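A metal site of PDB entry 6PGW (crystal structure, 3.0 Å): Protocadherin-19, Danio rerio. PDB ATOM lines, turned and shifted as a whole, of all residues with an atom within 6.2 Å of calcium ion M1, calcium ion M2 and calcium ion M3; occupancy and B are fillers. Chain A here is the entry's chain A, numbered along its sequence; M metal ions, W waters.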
ATOM      1  N   GLU A 230      -1.925   2.284  21.136  1.00  0.00           N
ATOM      2  CA  GLU A 230      -1.445   1.828  22.421  1.00  0.00           C
ATOM      3  C   GLU A 230      -1.192   3.044  23.339  1.00  0.00           C
ATOM      4  O   GLU A 230      -0.990   4.163  22.859  1.00  0.00           O
ATOM      5  CB  GLU A 230      -0.183   0.981  22.152  1.00  0.00           C
ATOM      6  CG  GLU A 230       0.807   0.878  23.250  1.00  0.00           C
ATOM      7  CD  GLU A 230       1.875  -0.150  22.962  1.00  0.00           C
ATOM      8  OE1 GLU A 230       2.432  -0.218  21.827  1.00  0.00           O
ATOM      9  OE2 GLU A 230       2.178  -0.875  23.884  1.00  0.00           O
ATOM     10  N   ASN A 231      -1.293   2.828  24.653  1.00  0.00           N
ATOM     11  CA  ASN A 231      -1.162   3.909  25.665  1.00  0.00           C
ATOM     12  C   ASN A 231      -2.232   5.033  25.539  1.00  0.00           C
ATOM     13  O   ASN A 231      -1.946   6.203  25.809  1.00  0.00           O
ATOM     14  CB  ASN A 231       0.248   4.532  25.628  1.00  0.00           C
ATOM     15  CG  ASN A 231       1.342   3.498  25.719  1.00  0.00           C
ATOM     16  OD1 ASN A 231       1.160   2.460  26.322  1.00  0.00           O
ATOM     17  ND2 ASN A 231       2.481   3.785  25.107  1.00  0.00           N
ATOM     18  N   PHE A 286      -4.560   0.718  27.147  1.00  0.00           N
ATOM     19  CA  PHE A 286      -4.180  -0.502  26.410  1.00  0.00           C
ATOM     20  C   PHE A 286      -2.662  -0.567  26.087  1.00  0.00           C
ATOM     21  O   PHE A 286      -1.980   0.455  25.972  1.00  0.00           O
ATOM     22  CB  PHE A 286      -4.992  -0.621  25.109  1.00  0.00           C
ATOM     23  CG  PHE A 286      -6.493  -0.645  25.310  1.00  0.00           C
ATOM     24  CD1 PHE A 286      -7.081  -1.235  26.418  1.00  0.00           C
ATOM     25  CD2 PHE A 286      -7.332  -0.124  24.326  1.00  0.00           C
ATOM     26  CE1 PHE A 286      -8.456  -1.256  26.563  1.00  0.00           C
ATOM     27  CE2 PHE A 286      -8.710  -0.144  24.481  1.00  0.00           C
ATOM     28  CZ  PHE A 286      -9.266  -0.708  25.596  1.00  0.00           C
ATOM     29  N   ASN A 287      -2.159  -1.789  25.917  1.00  0.00           N
ATOM     30  CA  ASN A 287      -0.737  -2.068  25.727  1.00  0.00           C
ATOM     31  C   ASN A 287      -0.544  -3.257  24.789  1.00  0.00           C
ATOM     32  O   ASN A 287      -0.682  -4.394  25.186  1.00  0.00           O
ATOM     33  CB  ASN A 287      -0.086  -2.380  27.059  1.00  0.00           C
ATOM     34  CG  ASN A 287       1.380  -2.777  26.907  1.00  0.00           C
ATOM     35  OD1 ASN A 287       1.995  -2.595  25.846  1.00  0.00           O
ATOM     36  ND2 ASN A 287       1.930  -3.312  27.981  1.00  0.00           N
ATOM     37  N   HIS A 288      -0.188  -2.947  23.545  1.00  0.00           N
ATOM     38  CA  HIS A 288       0.084  -3.915  22.479  1.00  0.00           C
ATOM     39  C   HIS A 288       0.996  -5.092  22.867  1.00  0.00           C
ATOM     40  O   HIS A 288       0.976  -6.153  22.257  1.00  0.00           O
ATOM     41  CB  HIS A 288       0.716  -3.152  21.333  1.00  0.00           C
ATOM     42  CG  HIS A 288       1.083  -3.997  20.167  1.00  0.00           C
ATOM     43  ND1 HIS A 288       0.333  -4.013  19.011  1.00  0.00           N
ATOM     44  CD2 HIS A 288       2.139  -4.815  19.945  1.00  0.00           C
ATOM     45  CE1 HIS A 288       0.894  -4.832  18.135  1.00  0.00           C
ATOM     46  NE2 HIS A 288       1.988  -5.337  18.681  1.00  0.00           N
ATOM     47  N   GLU A 289       1.814  -4.889  23.874  1.00  0.00           N
ATOM     48  CA  GLU A 289       2.672  -5.924  24.344  1.00  0.00           C
ATOM     49  C   GLU A 289       1.906  -6.890  25.324  1.00  0.00           C
ATOM     50  O   GLU A 289       2.407  -7.956  25.704  1.00  0.00           O
ATOM     51  CB  GLU A 289       3.882  -5.257  24.988  1.00  0.00           C
ATOM     52  CG  GLU A 289       4.876  -4.663  23.967  1.00  0.00           C
ATOM     53  CD  GLU A 289       4.369  -3.439  23.206  1.00  0.00           C
ATOM     54  OE1 GLU A 289       4.522  -3.329  21.964  1.00  0.00           O
ATOM     55  OE2 GLU A 289       3.808  -2.557  23.842  1.00  0.00           O
ATOM     56  N   LEU A 319      -2.909  -1.050  18.092  1.00  0.00           N
ATOM     57  CA  LEU A 319      -1.817  -0.725  17.208  1.00  0.00           C
ATOM     58  C   LEU A 319      -0.513  -0.456  17.971  1.00  0.00           C
ATOM     59  O   LEU A 319      -0.531  -0.010  19.106  1.00  0.00           O
ATOM     60  CB  LEU A 319      -2.176   0.493  16.411  1.00  0.00           C
ATOM     61  CG  LEU A 319      -3.486   0.424  15.622  1.00  0.00           C
ATOM     62  CD1 LEU A 319      -3.819   1.805  15.088  1.00  0.00           C
ATOM     63  CD2 LEU A 319      -3.414  -0.585  14.486  1.00  0.00           C
ATOM     64  N   ASP A 320       0.606  -0.724  17.324  1.00  0.00           N
ATOM     65  CA  ASP A 320       1.916  -0.669  17.967  1.00  0.00           C
ATOM     66  C   ASP A 320       2.433   0.747  17.922  1.00  0.00           C
ATOM     67  O   ASP A 320       2.417   1.396  16.858  1.00  0.00           O
ATOM     68  CB  ASP A 320       2.878  -1.612  17.245  1.00  0.00           C
ATOM     69  CG  ASP A 320       4.277  -1.684  17.899  1.00  0.00           C
ATOM     70  OD1 ASP A 320       4.402  -1.655  19.172  1.00  0.00           O
ATOM     71  OD2 ASP A 320       5.247  -1.792  17.112  1.00  0.00           O
ATOM     72  N   VAL A 321       2.888   1.217  19.067  1.00  0.00           N
ATOM     73  CA  VAL A 321       3.735   2.393  19.134  1.00  0.00           C
ATOM     74  C   VAL A 321       5.065   2.043  19.800  1.00  0.00           C
ATOM     75  O   VAL A 321       5.146   1.081  20.605  1.00  0.00           O
ATOM     76  CB  VAL A 321       3.039   3.580  19.838  1.00  0.00           C
ATOM     77  CG1 VAL A 321       1.653   3.806  19.254  1.00  0.00           C
ATOM     78  CG2 VAL A 321       2.949   3.350  21.347  1.00  0.00           C
ATOM     79  N   ASN A 322       6.089   2.816  19.421  1.00  0.00           N
ATOM     80  CA  ASN A 322       7.466   2.557  19.796  1.00  0.00           C
ATOM     81  C   ASN A 322       7.674   3.063  21.217  1.00  0.00           C
ATOM     82  O   ASN A 322       8.357   4.059  21.443  1.00  0.00           O
ATOM     83  CB  ASN A 322       8.451   3.245  18.813  1.00  0.00           C
ATOM     84  CG  ASN A 322       9.898   2.807  19.019  1.00  0.00           C
ATOM     85  OD1 ASN A 322      10.161   1.751  19.640  1.00  0.00           O
ATOM     86  ND2 ASN A 322      10.853   3.610  18.510  1.00  0.00           N
ATOM     87  N   ASP A 323       7.098   2.340  22.165  1.00  0.00           N
ATOM     88  CA  ASP A 323       7.002   2.762  23.553  1.00  0.00           C
ATOM     89  C   ASP A 323       7.829   1.866  24.418  1.00  0.00           C
ATOM     90  O   ASP A 323       7.641   1.778  25.626  1.00  0.00           O
ATOM     91  CB  ASP A 323       5.539   2.735  23.998  1.00  0.00           C
ATOM     92  CG  ASP A 323       4.907   1.321  24.007  1.00  0.00           C
ATOM     93  OD1 ASP A 323       5.271   0.412  23.174  1.00  0.00           O
ATOM     94  OD2 ASP A 323       4.003   1.135  24.839  1.00  0.00           O
ATOM     95  N   ASN A 324       8.755   1.180  23.770  1.00  0.00           N
ATOM     96  CA  ASN A 324       9.735   0.384  24.440  1.00  0.00           C
ATOM     97  C   ASN A 324      11.059   0.697  23.811  1.00  0.00           C
ATOM     98  O   ASN A 324      11.299   0.398  22.561  1.00  0.00           O
ATOM     99  CB  ASN A 324       9.473  -1.094  24.268  1.00  0.00           C
ATOM    100  CG  ASN A 324       8.358  -1.591  25.113  1.00  0.00           C
ATOM    101  OD1 ASN A 324       8.475  -1.680  26.322  1.00  0.00           O
ATOM    102  ND2 ASN A 324       7.274  -1.981  24.455  1.00  0.00           N
ATOM    103  N   THR A 325      11.887   1.355  24.630  1.00  0.00           N
ATOM    104  CA  THR A 325      13.334   1.469  24.433  1.00  0.00           C
ATOM    105  C   THR A 325      13.949   0.078  24.562  1.00  0.00           C
ATOM    106  O   THR A 325      13.592  -0.671  25.456  1.00  0.00           O
ATOM    107  CB  THR A 325      13.985   2.356  25.528  1.00  0.00           C
ATOM    108  OG1 THR A 325      13.430   1.995  26.799  1.00  0.00           O
ATOM    109  CG2 THR A 325      13.755   3.830  25.301  1.00  0.00           C
ATOM    110  N   PRO A 326      14.924  -0.237  23.684  1.00  0.00           N
ATOM    111  CA  PRO A 326      15.603  -1.553  23.655  1.00  0.00           C
ATOM    112  C   PRO A 326      16.357  -1.890  24.939  1.00  0.00           C
ATOM    113  O   PRO A 326      16.673  -0.995  25.704  1.00  0.00           O
ATOM    114  CB  PRO A 326      16.612  -1.399  22.522  1.00  0.00           C
ATOM    115  CG  PRO A 326      16.094  -0.299  21.677  1.00  0.00           C
ATOM    116  CD  PRO A 326      15.337   0.622  22.563  1.00  0.00           C
ATOM    117  N   ASP A 359      13.922  -5.923  22.138  1.00  0.00           N
ATOM    118  CA  ASP A 359      12.956  -4.765  22.074  1.00  0.00           C
ATOM    119  C   ASP A 359      11.592  -5.420  21.865  1.00  0.00           C
ATOM    120  O   ASP A 359      11.455  -6.333  21.053  1.00  0.00           O
ATOM    121  CB  ASP A 359      13.287  -3.821  20.895  1.00  0.00           C
ATOM    122  CG  ASP A 359      12.446  -2.515  20.874  1.00  0.00           C
ATOM    123  OD1 ASP A 359      11.228  -2.552  20.923  1.00  0.00           O
ATOM    124  OD2 ASP A 359      13.020  -1.464  20.689  1.00  0.00           O
ATOM    125  N   TYR A 360      10.587  -4.993  22.614  1.00  0.00           N
ATOM    126  CA  TYR A 360       9.306  -5.698  22.606  1.00  0.00           C
ATOM    127  C   TYR A 360       8.368  -5.288  21.551  1.00  0.00           C
ATOM    128  O   TYR A 360       7.530  -6.091  21.105  1.00  0.00           O
ATOM    129  CB  TYR A 360       8.645  -5.582  23.966  1.00  0.00           C
ATOM    130  CG  TYR A 360       9.575  -6.049  25.068  1.00  0.00           C
ATOM    131  CD1 TYR A 360      10.282  -7.254  24.950  1.00  0.00           C
ATOM    132  CD2 TYR A 360       9.814  -5.257  26.169  1.00  0.00           C
ATOM    133  CE1 TYR A 360      11.142  -7.677  25.939  1.00  0.00           C
ATOM    134  CE2 TYR A 360      10.689  -5.663  27.161  1.00  0.00           C
ATOM    135  CZ  TYR A 360      11.336  -6.882  27.037  1.00  0.00           C
ATOM    136  OH  TYR A 360      12.189  -7.278  28.010  1.00  0.00           O
ATOM    137  N   ASP A 361       8.511  -4.084  21.063  1.00  0.00           N
ATOM    138  CA  ASP A 361       7.621  -3.619  20.070  1.00  0.00           C
ATOM    139  C   ASP A 361       7.687  -4.541  18.849  1.00  0.00           C
ATOM    140  O   ASP A 361       8.596  -5.377  18.741  1.00  0.00           O
ATOM    141  CB  ASP A 361       7.930  -2.200  19.694  1.00  0.00           C
ATOM    142  CG  ASP A 361       7.883  -1.255  20.887  1.00  0.00           C
ATOM    143  OD1 ASP A 361       6.908  -1.351  21.708  1.00  0.00           O
ATOM    144  OD2 ASP A 361       8.824  -0.391  20.968  1.00  0.00           O
ATOM    145  N   GLU A 362       6.705  -4.443  17.986  1.00  0.00           N
ATOM    146  CA  GLU A 362       6.679  -5.275  16.787  1.00  0.00           C
ATOM    147  C   GLU A 362       7.030  -4.414  15.593  1.00  0.00           C
ATOM    148  O   GLU A 362       6.835  -3.208  15.610  1.00  0.00           O
ATOM    149  CB  GLU A 362       5.316  -5.907  16.619  1.00  0.00           C
ATOM    150  CG  GLU A 362       5.102  -6.647  15.286  1.00  0.00           C
ATOM    151  CD  GLU A 362       3.805  -6.257  14.595  1.00  0.00           C
ATOM    152  OE1 GLU A 362       3.563  -6.752  13.457  1.00  0.00           O
ATOM    153  OE2 GLU A 362       3.003  -5.491  15.189  1.00  0.00           O
ATOM    154  N   GLU A 364       9.069  -2.447  12.640  1.00  0.00           N
ATOM    155  CA  GLU A 364      10.174  -1.518  12.586  1.00  0.00           C
ATOM    156  C   GLU A 364      10.503  -1.039  13.976  1.00  0.00           C
ATOM    157  O   GLU A 364      11.658  -0.904  14.338  1.00  0.00           O
ATOM    158  CB  GLU A 364       9.835  -0.338  11.694  1.00  0.00           C
ATOM    159  CG  GLU A 364       9.633  -0.685  10.234  1.00  0.00           C
ATOM    160  CD  GLU A 364      10.944  -0.900   9.495  1.00  0.00           C
ATOM    161  OE1 GLU A 364      11.598   0.106   9.130  1.00  0.00           O
ATOM    162  OE2 GLU A 364      11.315  -2.083   9.288  1.00  0.00           O
ATOM    163  N   ASN A 365       9.462  -0.849  14.762  1.00  0.00           N
ATOM    164  CA  ASN A 365       9.580  -0.429  16.112  1.00  0.00           C
ATOM    165  C   ASN A 365      10.400  -1.367  16.907  1.00  0.00           C
ATOM    166  O   ASN A 365      10.966  -0.995  17.973  1.00  0.00           O
ATOM    167  CB  ASN A 365       8.236  -0.383  16.756  1.00  0.00           C
ATOM    168  CG  ASN A 365       7.360   0.713  16.200  1.00  0.00           C
ATOM    169  OD1 ASN A 365       6.763   1.464  16.945  1.00  0.00           O
ATOM    170  ND2 ASN A 365       7.282   0.802  14.886  1.00  0.00           N
ATOM    171  N   GLY A 366      10.392  -2.618  16.493  1.00  0.00           N
ATOM    172  CA  GLY A 366      11.100  -3.632  17.198  1.00  0.00           C
ATOM    173  C   GLY A 366      12.391  -4.084  16.606  1.00  0.00           C
ATOM    174  O   GLY A 366      13.020  -5.005  17.148  1.00  0.00           O
ATOM    175  N   ARG A 367      12.800  -3.468  15.491  1.00  0.00           N
ATOM    176  CA  ARG A 367      13.991  -3.939  14.754  1.00  0.00           C
ATOM    177  C   ARG A 367      15.258  -3.287  15.291  1.00  0.00           C
ATOM    178  O   ARG A 367      15.284  -2.058  15.545  1.00  0.00           O
ATOM    179  CB  ARG A 367      13.862  -3.646  13.273  1.00  0.00           C
ATOM    180  CG  ARG A 367      14.551  -4.675  12.368  1.00  0.00           C
ATOM    181  CD  ARG A 367      14.458  -4.274  10.908  1.00  0.00           C
ATOM    182  NE  ARG A 367      15.427  -3.235  10.534  1.00  0.00           N
ATOM    183  CZ  ARG A 367      15.122  -2.063  10.002  1.00  0.00           C
ATOM    184  NH1 ARG A 367      16.085  -1.228   9.660  1.00  0.00           N
ATOM    185  NH2 ARG A 367      13.855  -1.713   9.778  1.00  0.00           N
ATOM    186  N   ASP A 411      16.747   1.222  17.596  1.00  0.00           N
ATOM    187  CA  ASP A 411      15.655   0.585  16.838  1.00  0.00           C
ATOM    188  C   ASP A 411      15.175   1.452  15.654  1.00  0.00           C
ATOM    189  O   ASP A 411      15.842   2.445  15.305  1.00  0.00           O
ATOM    190  CB  ASP A 411      14.495   0.135  17.769  1.00  0.00           C
ATOM    191  CG  ASP A 411      13.654   1.306  18.323  1.00  0.00           C
ATOM    192  OD1 ASP A 411      13.948   2.487  17.992  1.00  0.00           O
ATOM    193  OD2 ASP A 411      12.684   1.010  19.127  1.00  0.00           O
ATOM    194  N   LEU A 417      14.123   4.712  19.421  1.00  0.00           N
ATOM    195  CA  LEU A 417      14.664   4.581  20.770  1.00  0.00           C
ATOM    196  C   LEU A 417      15.979   3.787  20.723  1.00  0.00           C
ATOM    197  O   LEU A 417      16.339   3.271  19.653  1.00  0.00           O
ATOM    198  CB  LEU A 417      13.642   3.954  21.744  1.00  0.00           C
ATOM    199  CG  LEU A 417      12.576   4.894  22.392  1.00  0.00           C
ATOM    200  CD1 LEU A 417      13.187   6.190  22.929  1.00  0.00           C
ATOM    201  CD2 LEU A 417      11.471   5.232  21.408  1.00  0.00           C
HETATM  202 CA    CA M   1      11.059  -0.284  20.284  1.00  0.00          CA
HETATM  203 CA    CA M   2       4.592  -1.051  21.431  1.00  0.00          CA
HETATM  204 CA    CA M   3       3.720  -1.037  25.566  1.00  0.00          CA
HETATM  205  O   HOH W   1       2.081   0.160  26.656  1.00  0.00           O
HETATM  206  O   HOH W   2       5.619  -1.695  26.714  1.00  0.00           O
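The side-chain carboxylate (OE2) of Glu 230 lies close to the backbone NH (N) of His 288 (3.2 Å). The backbone NH (N) of Glu 230 lies close to the backbone carbonyl oxygen (O) of Leu 319, at 3.4 Å. The side-chain amide nitrogen of Asn 324 sits close to the side-chain carboxylate of Asp 323, at 3.4 Å. The side-chain carboxylate (OD2) of Asp 323 sits close to the side-chain amide nitrogen (ND2) of Asn 231, 3.1 Å away. OD2 of Asp 320 lies within hydrogen-bond range of N of Glu 362. OD1 of Asp 411 is in hydrogen-bond range of N of Leu 417 (2.7 Å).
Six residues have an atom within 4 Å of calcium ion M1: Asn 322, Asn 324, Asp 359, Asp 361, Asn 365 and Asp 411. The nearest printed residue that does not touch calcium ion M1 is Gly 366 (4.5 Å).
Six residues have an atom within 4 Å of calcium ion M2: Glu 230, Glu 289, Asp 320, Val 321, Asp 323 and Asp 361.
Five residues have an atom within 4 Å of calcium ion M3: Glu 230, Asn 287, Glu 289, Asp 323 and Asn 324.
OD1 of Asn 322 binds calcium ion M1. Calcium ion M1 is bound by OD2 of Asp 359 (2.3 Å). Calcium ion M1 is bound by OD2 of Asp 361 (2.3 Å). OD1 of Asp 359 binds calcium ion M1 (2.4 Å). OD2 of Asp 411 is bound to calcium ion M1, 2.4 Å away. Calcium ion M1 is bound by O of Asn 324, at 2.4 Å. O of Asn 365 is bound to calcium ion M1, at 2.4 Å. Calcium ion M1 has seven donor atoms within binding distance.
Calcium ion M2 is bound by the side-chain carboxylate (OE1) of Glu 289 (2.3 Å), the side-chain carboxylate (OD1) of Asp 320 (2.3 Å), the side-chain carboxylate (OE1) of Glu 230 (2.3 Å), the side-chain carboxylate (OD1) of Asp 361 (2.4 Å), the backbone carbonyl oxygen (O) of Val 321 (2.4 Å) and the side-chain carboxylate (OD1) of Asp 323 (2.4 Å). Calcium ion M2 has six donor atoms within binding distance. Slightly farther from calcium ion M2 lies OE2 of Glu 289 (2.9 Å).
Calcium ion M3 is bound by OE2 of Glu 230, OE2 of Glu 289, water W1, OD2 of Asp 323, water W2 and OD1 of Asn 287.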
